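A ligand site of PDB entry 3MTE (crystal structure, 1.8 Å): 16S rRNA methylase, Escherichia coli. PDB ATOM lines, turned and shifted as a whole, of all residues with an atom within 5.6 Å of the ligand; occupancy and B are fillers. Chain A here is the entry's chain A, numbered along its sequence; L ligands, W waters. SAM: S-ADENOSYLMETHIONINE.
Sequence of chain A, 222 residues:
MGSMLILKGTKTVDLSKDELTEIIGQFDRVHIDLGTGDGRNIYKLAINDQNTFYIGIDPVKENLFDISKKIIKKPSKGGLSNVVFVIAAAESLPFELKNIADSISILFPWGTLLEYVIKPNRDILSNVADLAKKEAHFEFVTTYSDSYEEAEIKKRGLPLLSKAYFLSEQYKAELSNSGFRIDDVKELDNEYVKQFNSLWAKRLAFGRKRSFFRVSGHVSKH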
ATOM      1  N   ASP A  33      -6.694 -20.141   0.949  1.00  0.00           N
ATOM      2  CA  ASP A  33      -5.351 -19.885   0.398  1.00  0.00           C
ATOM      3  C   ASP A  33      -5.467 -18.700  -0.580  1.00  0.00           C
ATOM      4  O   ASP A  33      -6.120 -18.816  -1.624  1.00  0.00           O
ATOM      5  CB  ASP A  33      -4.832 -21.132  -0.315  1.00  0.00           C
ATOM      6  CG  ASP A  33      -3.404 -20.988  -0.832  1.00  0.00           C
ATOM      7  OD1 ASP A  33      -2.567 -20.355  -0.143  1.00  0.00           O
ATOM      8  OD2 ASP A  33      -3.119 -21.513  -1.928  1.00  0.00           O
ATOM      9  N   LEU A  34      -4.863 -17.570  -0.233  1.00  0.00           N
ATOM     10  CA  LEU A  34      -5.003 -16.347  -1.009  1.00  0.00           C
ATOM     11  C   LEU A  34      -3.858 -16.211  -2.027  1.00  0.00           C
ATOM     12  O   LEU A  34      -2.697 -16.343  -1.664  1.00  0.00           O
ATOM     13  CB  LEU A  34      -5.016 -15.119  -0.078  1.00  0.00           C
ATOM     14  CG  LEU A  34      -5.091 -13.731  -0.731  1.00  0.00           C
ATOM     15  CD1 LEU A  34      -6.360 -13.554  -1.594  1.00  0.00           C
ATOM     16  CD2 LEU A  34      -5.015 -12.657   0.342  1.00  0.00           C
ATOM     17  N   GLY A  35      -4.197 -15.929  -3.277  1.00  0.00           N
ATOM     18  CA  GLY A  35      -3.186 -15.912  -4.330  1.00  0.00           C
ATOM     19  C   GLY A  35      -2.709 -17.329  -4.574  1.00  0.00           C
ATOM     20  O   GLY A  35      -1.491 -17.611  -4.548  1.00  0.00           O
ATOM     21  N   THR A  36      -3.680 -18.217  -4.822  1.00  0.00           N
ATOM     22  CA  THR A  36      -3.464 -19.666  -4.813  1.00  0.00           C
ATOM     23  C   THR A  36      -2.712 -20.184  -6.047  1.00  0.00           C
ATOM     24  O   THR A  36      -2.087 -21.252  -6.001  1.00  0.00           O
ATOM     25  CB  THR A  36      -4.806 -20.457  -4.583  1.00  0.00           C
ATOM     26  OG1 THR A  36      -4.517 -21.778  -4.112  1.00  0.00           O
ATOM     27  CG2 THR A  36      -5.620 -20.525  -5.864  1.00  0.00           C
ATOM     28  N   GLY A  37      -2.720 -19.414  -7.136  1.00  0.00           N
ATOM     29  CA  GLY A  37      -1.885 -19.754  -8.287  1.00  0.00           C
ATOM     30  C   GLY A  37      -2.528 -20.830  -9.160  1.00  0.00           C
ATOM     31  O   GLY A  37      -3.677 -20.671  -9.580  1.00  0.00           O
ATOM     32  N   ASP A  38      -1.818 -21.936  -9.404  1.00  0.00           N
ATOM     33  CA  ASP A  38      -2.318 -22.957 -10.334  1.00  0.00           C
ATOM     34  C   ASP A  38      -3.274 -23.979  -9.698  1.00  0.00           C
ATOM     35  O   ASP A  38      -3.800 -24.863 -10.395  1.00  0.00           O
ATOM     36  CB  ASP A  38      -1.175 -23.649 -11.123  1.00  0.00           C
ATOM     37  CG  ASP A  38      -0.221 -24.461 -10.239  1.00  0.00           C
ATOM     38  OD1 ASP A  38      -0.565 -24.773  -9.077  1.00  0.00           O
ATOM     39  OD2 ASP A  38       0.891 -24.788 -10.726  1.00  0.00           O
ATOM     40  N   ASN A  41      -1.297 -26.759  -5.171  1.00  0.00           N
ATOM     41  CA  ASN A  41      -1.089 -26.828  -3.726  1.00  0.00           C
ATOM     42  C   ASN A  41      -2.377 -27.196  -3.010  1.00  0.00           C
ATOM     43  O   ASN A  41      -2.400 -28.115  -2.194  1.00  0.00           O
ATOM     44  CB  ASN A  41      -0.579 -25.495  -3.190  1.00  0.00           C
ATOM     45  CG  ASN A  41       0.861 -25.217  -3.571  1.00  0.00           C
ATOM     46  OD1 ASN A  41       1.623 -26.134  -3.883  1.00  0.00           O
ATOM     47  ND2 ASN A  41       1.243 -23.937  -3.566  1.00  0.00           N
ATOM     48  N   ILE A  57      -8.186 -18.644  -3.654  1.00  0.00           N
ATOM     49  CA  ILE A  57      -8.558 -17.369  -4.259  1.00  0.00           C
ATOM     50  C   ILE A  57      -7.443 -16.911  -5.188  1.00  0.00           C
ATOM     51  O   ILE A  57      -6.269 -16.871  -4.785  1.00  0.00           O
ATOM     52  CB  ILE A  57      -8.728 -16.279  -3.176  1.00  0.00           C
ATOM     53  CG1 ILE A  57      -9.752 -16.716  -2.123  1.00  0.00           C
ATOM     54  CG2 ILE A  57      -9.142 -14.971  -3.821  1.00  0.00           C
ATOM     55  CD1 ILE A  57      -9.960 -15.691  -1.032  1.00  0.00           C
ATOM     56  N   ASP A  58      -7.808 -16.587  -6.426  1.00  0.00           N
ATOM     57  CA  ASP A  58      -6.854 -15.985  -7.371  1.00  0.00           C
ATOM     58  C   ASP A  58      -7.578 -15.085  -8.359  1.00  0.00           C
ATOM     59  O   ASP A  58      -8.714 -15.387  -8.790  1.00  0.00           O
ATOM     60  CB  ASP A  58      -6.051 -17.057  -8.117  1.00  0.00           C
ATOM     61  CG  ASP A  58      -4.689 -16.531  -8.608  1.00  0.00           C
ATOM     62  OD1 ASP A  58      -3.672 -16.786  -7.923  1.00  0.00           O
ATOM     63  OD2 ASP A  58      -4.629 -15.851  -9.652  1.00  0.00           O
ATOM     64  N   PRO A  59      -6.955 -13.956  -8.709  1.00  0.00           N
ATOM     65  CA  PRO A  59      -7.540 -13.001  -9.653  1.00  0.00           C
ATOM     66  C   PRO A  59      -7.418 -13.421 -11.113  1.00  0.00           C
ATOM     67  O   PRO A  59      -8.120 -12.856 -11.962  1.00  0.00           O
ATOM     68  CB  PRO A  59      -6.736 -11.708  -9.402  1.00  0.00           C
ATOM     69  CG  PRO A  59      -5.457 -12.157  -8.807  1.00  0.00           C
ATOM     70  CD  PRO A  59      -5.799 -13.389  -7.981  1.00  0.00           C
ATOM     71  N   VAL A  60      -6.545 -14.366 -11.420  1.00  0.00           N
ATOM     72  CA  VAL A  60      -6.363 -14.793 -12.808  1.00  0.00           C
ATOM     73  C   VAL A  60      -6.935 -16.198 -13.001  1.00  0.00           C
ATOM     74  O   VAL A  60      -6.309 -17.202 -12.676  1.00  0.00           O
ATOM     75  CB  VAL A  60      -4.874 -14.759 -13.239  1.00  0.00           C
ATOM     76  CG1 VAL A  60      -4.759 -14.996 -14.742  1.00  0.00           C
ATOM     77  CG2 VAL A  60      -4.261 -13.396 -12.848  1.00  0.00           C
ATOM     78  N   ASN A  63      -5.187 -19.309 -14.717  1.00  0.00           N
ATOM     79  CA  ASN A  63      -4.155 -20.020 -13.958  1.00  0.00           C
ATOM     80  C   ASN A  63      -4.723 -21.308 -13.365  1.00  0.00           C
ATOM     81  O   ASN A  63      -4.004 -22.271 -13.101  1.00  0.00           O
ATOM     82  CB  ASN A  63      -3.654 -19.165 -12.794  1.00  0.00           C
ATOM     83  CG  ASN A  63      -2.786 -18.001 -13.223  1.00  0.00           C
ATOM     84  OD1 ASN A  63      -2.377 -17.894 -14.374  1.00  0.00           O
ATOM     85  ND2 ASN A  63      -2.475 -17.125 -12.272  1.00  0.00           N
ATOM     86  N   ALA A  88     -11.000 -13.563  -7.357  1.00  0.00           N
ATOM     87  CA  ALA A  88     -11.010 -12.256  -6.718  1.00  0.00           C
ATOM     88  C   ALA A  88      -9.580 -11.842  -6.411  1.00  0.00           C
ATOM     89  O   ALA A  88      -8.664 -12.663  -6.433  1.00  0.00           O
ATOM     90  CB  ALA A  88     -11.825 -12.297  -5.418  1.00  0.00           C
ATOM     91  N   ALA A  89      -9.386 -10.555  -6.147  1.00  0.00           N
ATOM     92  CA  ALA A  89      -8.100 -10.036  -5.727  1.00  0.00           C
ATOM     93  C   ALA A  89      -8.131  -9.595  -4.265  1.00  0.00           C
ATOM     94  O   ALA A  89      -9.197  -9.280  -3.727  1.00  0.00           O
ATOM     95  CB  ALA A  89      -7.677  -8.870  -6.620  1.00  0.00           C
ATOM     96  N   ALA A  90      -6.951  -9.558  -3.649  1.00  0.00           N
ATOM     97  CA  ALA A  90      -6.787  -9.101  -2.280  1.00  0.00           C
ATOM     98  C   ALA A  90      -7.391  -7.716  -2.022  1.00  0.00           C
ATOM     99  O   ALA A  90      -7.863  -7.449  -0.917  1.00  0.00           O
ATOM    100  CB  ALA A  90      -5.283  -9.120  -1.886  1.00  0.00           C
ATOM    101  N   GLU A  91      -7.371  -6.846  -3.036  1.00  0.00           N
ATOM    102  CA  GLU A  91      -7.855  -5.467  -2.863  1.00  0.00           C
ATOM    103  C   GLU A  91      -9.370  -5.388  -2.874  1.00  0.00           C
ATOM    104  O   GLU A  91      -9.941  -4.342  -2.543  1.00  0.00           O
ATOM    105  CB  GLU A  91      -7.343  -4.533  -3.975  1.00  0.00           C
ATOM    106  CG  GLU A  91      -5.924  -4.734  -4.416  1.00  0.00           C
ATOM    107  CD  GLU A  91      -5.797  -5.854  -5.442  1.00  0.00           C
ATOM    108  OE1 GLU A  91      -6.008  -5.628  -6.662  1.00  0.00           O
ATOM    109  OE2 GLU A  91      -5.485  -6.952  -5.011  1.00  0.00           O
ATOM    110  N   LEU A 107       1.025 -18.022   0.132  1.00  0.00           N
ATOM    111  CA  LEU A 107       2.239 -18.785  -0.178  1.00  0.00           C
ATOM    112  C   LEU A 107       2.932 -18.274  -1.440  1.00  0.00           C
ATOM    113  O   LEU A 107       2.346 -18.274  -2.515  1.00  0.00           O
ATOM    114  CB  LEU A 107       1.912 -20.260  -0.389  1.00  0.00           C
ATOM    115  CG  LEU A 107       1.111 -20.943   0.732  1.00  0.00           C
ATOM    116  CD1 LEU A 107       0.703 -22.347   0.297  1.00  0.00           C
ATOM    117  CD2 LEU A 107       1.934 -21.002   2.018  1.00  0.00           C
ATOM    118  N   PHE A 108       4.184 -17.862  -1.279  1.00  0.00           N
ATOM    119  CA  PHE A 108       4.997 -17.363  -2.389  1.00  0.00           C
ATOM    120  C   PHE A 108       4.309 -16.254  -3.188  1.00  0.00           C
ATOM    121  O   PHE A 108       4.277 -16.299  -4.397  1.00  0.00           O
ATOM    122  CB  PHE A 108       5.426 -18.546  -3.279  1.00  0.00           C
ATOM    123  CG  PHE A 108       5.984 -19.691  -2.498  1.00  0.00           C
ATOM    124  CD1 PHE A 108       7.275 -19.640  -1.965  1.00  0.00           C
ATOM    125  CD2 PHE A 108       5.212 -20.822  -2.250  1.00  0.00           C
ATOM    126  CE1 PHE A 108       7.782 -20.708  -1.223  1.00  0.00           C
ATOM    127  CE2 PHE A 108       5.716 -21.882  -1.512  1.00  0.00           C
ATOM    128  CZ  PHE A 108       6.998 -21.818  -0.996  1.00  0.00           C
ATOM    129  N   PRO A 109       3.755 -15.252  -2.491  1.00  0.00           N
ATOM    130  CA  PRO A 109       3.147 -14.166  -3.266  1.00  0.00           C
ATOM    131  C   PRO A 109       4.198 -13.416  -4.058  1.00  0.00           C
ATOM    132  O   PRO A 109       5.385 -13.423  -3.688  1.00  0.00           O
ATOM    133  CB  PRO A 109       2.555 -13.251  -2.185  1.00  0.00           C
ATOM    134  CG  PRO A 109       3.440 -13.474  -0.997  1.00  0.00           C
ATOM    135  CD  PRO A 109       3.787 -14.948  -1.051  1.00  0.00           C
ATOM    136  N   TRP A 110       3.793 -12.769  -5.141  1.00  0.00           N
ATOM    137  CA  TRP A 110       4.724 -11.912  -5.865  1.00  0.00           C
ATOM    138  C   TRP A 110       4.073 -10.598  -6.229  1.00  0.00           C
ATOM    139  O   TRP A 110       2.891 -10.399  -5.936  1.00  0.00           O
ATOM    140  CB  TRP A 110       5.283 -12.605  -7.108  1.00  0.00           C
ATOM    141  CG  TRP A 110       4.271 -12.956  -8.190  1.00  0.00           C
ATOM    142  CD1 TRP A 110       3.036 -12.417  -8.395  1.00  0.00           C
ATOM    143  CD2 TRP A 110       4.465 -13.927  -9.230  1.00  0.00           C
ATOM    144  NE1 TRP A 110       2.442 -12.998  -9.503  1.00  0.00           N
ATOM    145  CE2 TRP A 110       3.296 -13.936 -10.025  1.00  0.00           C
ATOM    146  CE3 TRP A 110       5.511 -14.796  -9.559  1.00  0.00           C
ATOM    147  CZ2 TRP A 110       3.152 -14.775 -11.123  1.00  0.00           C
ATOM    148  CZ3 TRP A 110       5.358 -15.635 -10.646  1.00  0.00           C
ATOM    149  CH2 TRP A 110       4.198 -15.607 -11.425  1.00  0.00           C
ATOM    150  N   THR A 112       2.399  -7.131  -6.533  1.00  0.00           N
ATOM    151  CA  THR A 112       1.709  -6.253  -5.603  1.00  0.00           C
ATOM    152  C   THR A 112       1.305  -6.949  -4.313  1.00  0.00           C
ATOM    153  O   THR A 112       1.415  -6.354  -3.232  1.00  0.00           O
ATOM    154  CB  THR A 112       0.493  -5.587  -6.266  1.00  0.00           C
ATOM    155  OG1 THR A 112      -0.416  -6.597  -6.755  1.00  0.00           O
ATOM    156  CG2 THR A 112       0.983  -4.719  -7.414  1.00  0.00           C
ATOM    157  N   LEU A 113       0.886  -8.205  -4.409  1.00  0.00           N
ATOM    158  CA  LEU A 113       0.518  -8.978  -3.215  1.00  0.00           C
ATOM    159  C   LEU A 113       1.699  -9.146  -2.269  1.00  0.00           C
ATOM    160  O   LEU A 113       1.558  -9.046  -1.045  1.00  0.00           O
ATOM    161  CB  LEU A 113       0.002 -10.365  -3.604  1.00  0.00           C
ATOM    162  CG  LEU A 113      -0.506 -11.236  -2.444  1.00  0.00           C
ATOM    163  CD1 LEU A 113      -1.639 -10.529  -1.684  1.00  0.00           C
ATOM    164  CD2 LEU A 113      -0.963 -12.603  -2.952  1.00  0.00           C
ATOM    165  N   TYR A 116       2.153  -6.008  -0.379  1.00  0.00           N
ATOM    166  CA  TYR A 116       1.147  -5.825   0.678  1.00  0.00           C
ATOM    167  C   TYR A 116       1.552  -6.583   1.935  1.00  0.00           C
ATOM    168  O   TYR A 116       1.304  -6.135   3.057  1.00  0.00           O
ATOM    169  CB  TYR A 116      -0.228  -6.345   0.246  1.00  0.00           C
ATOM    170  CG  TYR A 116      -0.862  -5.711  -0.979  1.00  0.00           C
ATOM    171  CD1 TYR A 116      -0.601  -4.395  -1.326  1.00  0.00           C
ATOM    172  CD2 TYR A 116      -1.779  -6.429  -1.762  1.00  0.00           C
ATOM    173  CE1 TYR A 116      -1.191  -3.816  -2.435  1.00  0.00           C
ATOM    174  CE2 TYR A 116      -2.382  -5.846  -2.873  1.00  0.00           C
ATOM    175  CZ  TYR A 116      -2.087  -4.551  -3.198  1.00  0.00           C
ATOM    176  OH  TYR A 116      -2.673  -3.976  -4.294  1.00  0.00           O
ATOM    177  N   SER A 145      10.787 -13.343  -6.237  1.00  0.00           N
ATOM    178  CA  SER A 145      10.553 -14.246  -7.373  1.00  0.00           C
ATOM    179  C   SER A 145      11.750 -14.334  -8.305  1.00  0.00           C
ATOM    180  O   SER A 145      12.029 -15.386  -8.872  1.00  0.00           O
ATOM    181  CB  SER A 145       9.345 -13.772  -8.189  1.00  0.00           C
ATOM    182  OG  SER A 145       8.168 -13.761  -7.385  1.00  0.00           O
ATOM    183  N   SER A 198       2.822 -26.938  -6.534  1.00  0.00           N
ATOM    184  CA  SER A 198       2.631 -26.032  -7.658  1.00  0.00           C
ATOM    185  C   SER A 198       3.849 -26.002  -8.569  1.00  0.00           C
ATOM    186  O   SER A 198       4.968 -26.266  -8.133  1.00  0.00           O
ATOM    187  CB  SER A 198       2.294 -24.613  -7.179  1.00  0.00           C
ATOM    188  OG  SER A 198       3.417 -23.975  -6.598  1.00  0.00           O
ATOM    189  N   TRP A 200       5.183 -23.361  -9.850  1.00  0.00           N
ATOM    190  CA  TRP A 200       6.015 -22.255  -9.387  1.00  0.00           C
ATOM    191  C   TRP A 200       6.880 -22.669  -8.196  1.00  0.00           C
ATOM    192  O   TRP A 200       8.083 -22.378  -8.157  1.00  0.00           O
ATOM    193  CB  TRP A 200       5.148 -21.040  -9.031  1.00  0.00           C
ATOM    194  CG  TRP A 200       5.945 -19.871  -8.554  1.00  0.00           C
ATOM    195  CD1 TRP A 200       5.911 -19.309  -7.316  1.00  0.00           C
ATOM    196  CD2 TRP A 200       6.919 -19.131  -9.310  1.00  0.00           C
ATOM    197  NE1 TRP A 200       6.787 -18.243  -7.254  1.00  0.00           N
ATOM    198  CE2 TRP A 200       7.426 -18.133  -8.458  1.00  0.00           C
ATOM    199  CE3 TRP A 200       7.421 -19.231 -10.605  1.00  0.00           C
ATOM    200  CZ2 TRP A 200       8.389 -17.220  -8.876  1.00  0.00           C
ATOM    201  CZ3 TRP A 200       8.379 -18.331 -11.017  1.00  0.00           C
ATOM    202  CH2 TRP A 200       8.868 -17.336 -10.153  1.00  0.00           C
ATOM    203  N   ALA A 201       6.281 -23.346  -7.219  1.00  0.00           N
ATOM    204  CA  ALA A 201       7.053 -23.820  -6.080  1.00  0.00           C
ATOM    205  C   ALA A 201       8.152 -24.807  -6.506  1.00  0.00           C
ATOM    206  O   ALA A 201       9.265 -24.755  -5.989  1.00  0.00           O
ATOM    207  CB  ALA A 201       6.130 -24.452  -5.031  1.00  0.00           C
HETATM  208  N   SAM L   1       0.437 -19.559  -3.967  1.00  0.00           N
HETATM  209  CA  SAM L   1       0.989 -19.821  -5.295  1.00  0.00           C
HETATM  210  C   SAM L   1       1.937 -21.013  -5.260  1.00  0.00           C
HETATM  211  OXT SAM L   1       2.395 -21.422  -4.191  1.00  0.00           O
HETATM  212  CB  SAM L   1       1.737 -18.603  -5.840  1.00  0.00           C
HETATM  213  CG  SAM L   1       1.665 -18.523  -7.354  1.00  0.00           C
HETATM  214  SD  SAM L   1       2.333 -16.974  -8.015  1.00  0.00           S
HETATM  215  CE  SAM L   1       3.960 -16.939  -7.235  1.00  0.00           C
HETATM  216  C5' SAM L   1       1.494 -15.680  -7.076  1.00  0.00           C
HETATM  217  C4' SAM L   1      -0.015 -15.640  -7.324  1.00  0.00           C
HETATM  218  O4' SAM L   1      -0.533 -14.517  -6.640  1.00  0.00           O
HETATM  219  C3' SAM L   1      -0.422 -15.492  -8.777  1.00  0.00           C
HETATM  220  O3' SAM L   1      -1.344 -16.490  -9.128  1.00  0.00           O
HETATM  221  C2' SAM L   1      -1.178 -14.176  -8.856  1.00  0.00           C
HETATM  222  O2' SAM L   1      -2.253 -14.203  -9.784  1.00  0.00           O
HETATM  223  C1' SAM L   1      -1.601 -13.984  -7.404  1.00  0.00           C
HETATM  224  N9  SAM L   1      -1.783 -12.546  -7.119  1.00  0.00           N
HETATM  225  C8  SAM L   1      -1.009 -11.497  -7.539  1.00  0.00           C
HETATM  226  N7  SAM L   1      -1.556 -10.361  -7.051  1.00  0.00           N
HETATM  227  C5  SAM L   1      -2.655 -10.682  -6.331  1.00  0.00           C
HETATM  228  C6  SAM L   1      -3.582  -9.913  -5.631  1.00  0.00           C
HETATM  229  N6  SAM L   1      -3.473  -8.592  -5.584  1.00  0.00           N
HETATM  230  N1  SAM L   1      -4.613 -10.561  -4.976  1.00  0.00           N
HETATM  231  C2  SAM L   1      -4.755 -11.934  -5.020  1.00  0.00           C
HETATM  232  N3  SAM L   1      -3.827 -12.678  -5.722  1.00  0.00           N
HETATM  233  C4  SAM L   1      -2.806 -12.055  -6.365  1.00  0.00           C
HETATM  234  O   HOH W   1      -1.013 -18.640  -1.597  1.00  0.00           O
HETATM  235  O   HOH W   2      -0.997 -21.973  -3.396  1.00  0.00           O
HETATM  236  O   HOH W   3      -1.011 -14.652 -12.228  1.00  0.00           O
HETATM  237  O   HOH W   4       0.910 -21.558  -8.600  1.00  0.00           O
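The backbone NH (N) of Ala 90 lies within hydrogen-bond range of a nitrogen (N1) of the ligand, 2.9 Å away. The backbone carbonyl oxygen (O) of Leu 107 sits at hydrogen-bond distance from a nitrogen (N) of the ligand. OE2 of Glu 91 is in hydrogen-bond range of N6 of the ligand. O3' of the ligand lies within hydrogen-bond range of OD1 of Asp 58 (2.6 Å). An oxygen (O3') of the ligand sits at hydrogen-bond distance from the side-chain amide nitrogen (ND2) of Asn 63. ND2 of Asn 41 sits at hydrogen-bond distance from OXT of the ligand, at 2.8 Å. The backbone carbonyl oxygen of Gly 35 is in hydrogen-bond range of a nitrogen (N) of the ligand.
The backbone NH of Thr 36 sits at hydrogen-bond distance from the backbone carbonyl oxygen of Ile 57, 2.9 Å away. OD1 of Asp 58 is in hydrogen-bond range of N of Thr 36, 3.4 Å away. O of Asp 58 lies within hydrogen-bond range of N of Ala 88 (3.3 Å). The side-chain carboxylate (OD2) of Asp 33 is in hydrogen-bond range of the side-chain hydroxyl (OG1) of Thr 36 (2.6 Å). The backbone NH (N) of Ser 198 sits at hydrogen-bond distance from the side-chain amide oxygen (OD1) of Asn 41 (3.0 Å). The side-chain carboxylate (OD2) of Asp 58 is in hydrogen-bond range of the backbone NH (N) of Val 60 (3.0 Å). The backbone NH of Ala 201 sits at hydrogen-bond distance from the side-chain hydroxyl of Ser 198 (3.0 Å). N of Gly 37 sits at hydrogen-bond distance from OD1 of Asp 58.
Thr 36 touches the ligand. CA of Gly 37 touches O3' of the ligand (3.4 Å). Pro 59 touches the ligand. CG2 of Val 60 touches O2' of the ligand, 3.8 Å away. CA of Ala 89 touches N1 of the ligand, at 3.6 Å. Phe 108 touches the ligand (O to CE, 2.9 Å). CE3 of Trp 110 touches CE of the ligand, at 3.5 Å. Thr 112 touches the ligand (OG1 to N6, 3.8 Å). Leu 113 touches the ligand (CB to N7, 3.8 Å). Ser 198 touches the ligand (OG to C, 3.6 Å). CD1 of Trp 200 touches CE of the ligand, 3.1 Å away. Hydrophobic or aromatic side chains within 4 Å of the ligand: Pro 59, Val 60, Ala 89, Ala 90, Leu 107, Phe 108, Trp 110, Leu 113 and Trp 200. Within 4 Å of the ligand: Gly 35, Thr 36, Gly 37, Asn 41, Asp 58, Pro 59, Val 60, Asn 63, Ala 89, Ala 90, Glu 91, Leu 107, Phe 108, Trp 110, Thr 112, Leu 113, Ser 198 and Trp 200.
Water W3 bridges O2' of the ligand and ND2 of Asn 63. Water W2 lies within hydrogen-bond range of the side-chain carboxylate (OD2) of Asp 33 (2.6 Å), a nitrogen (N) of the ligand (2.9 Å), the backbone carbonyl oxygen (O) of Thr 36 (2.9 Å) and the side-chain amide nitrogen (ND2) of Asn 41 (3.0 Å).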
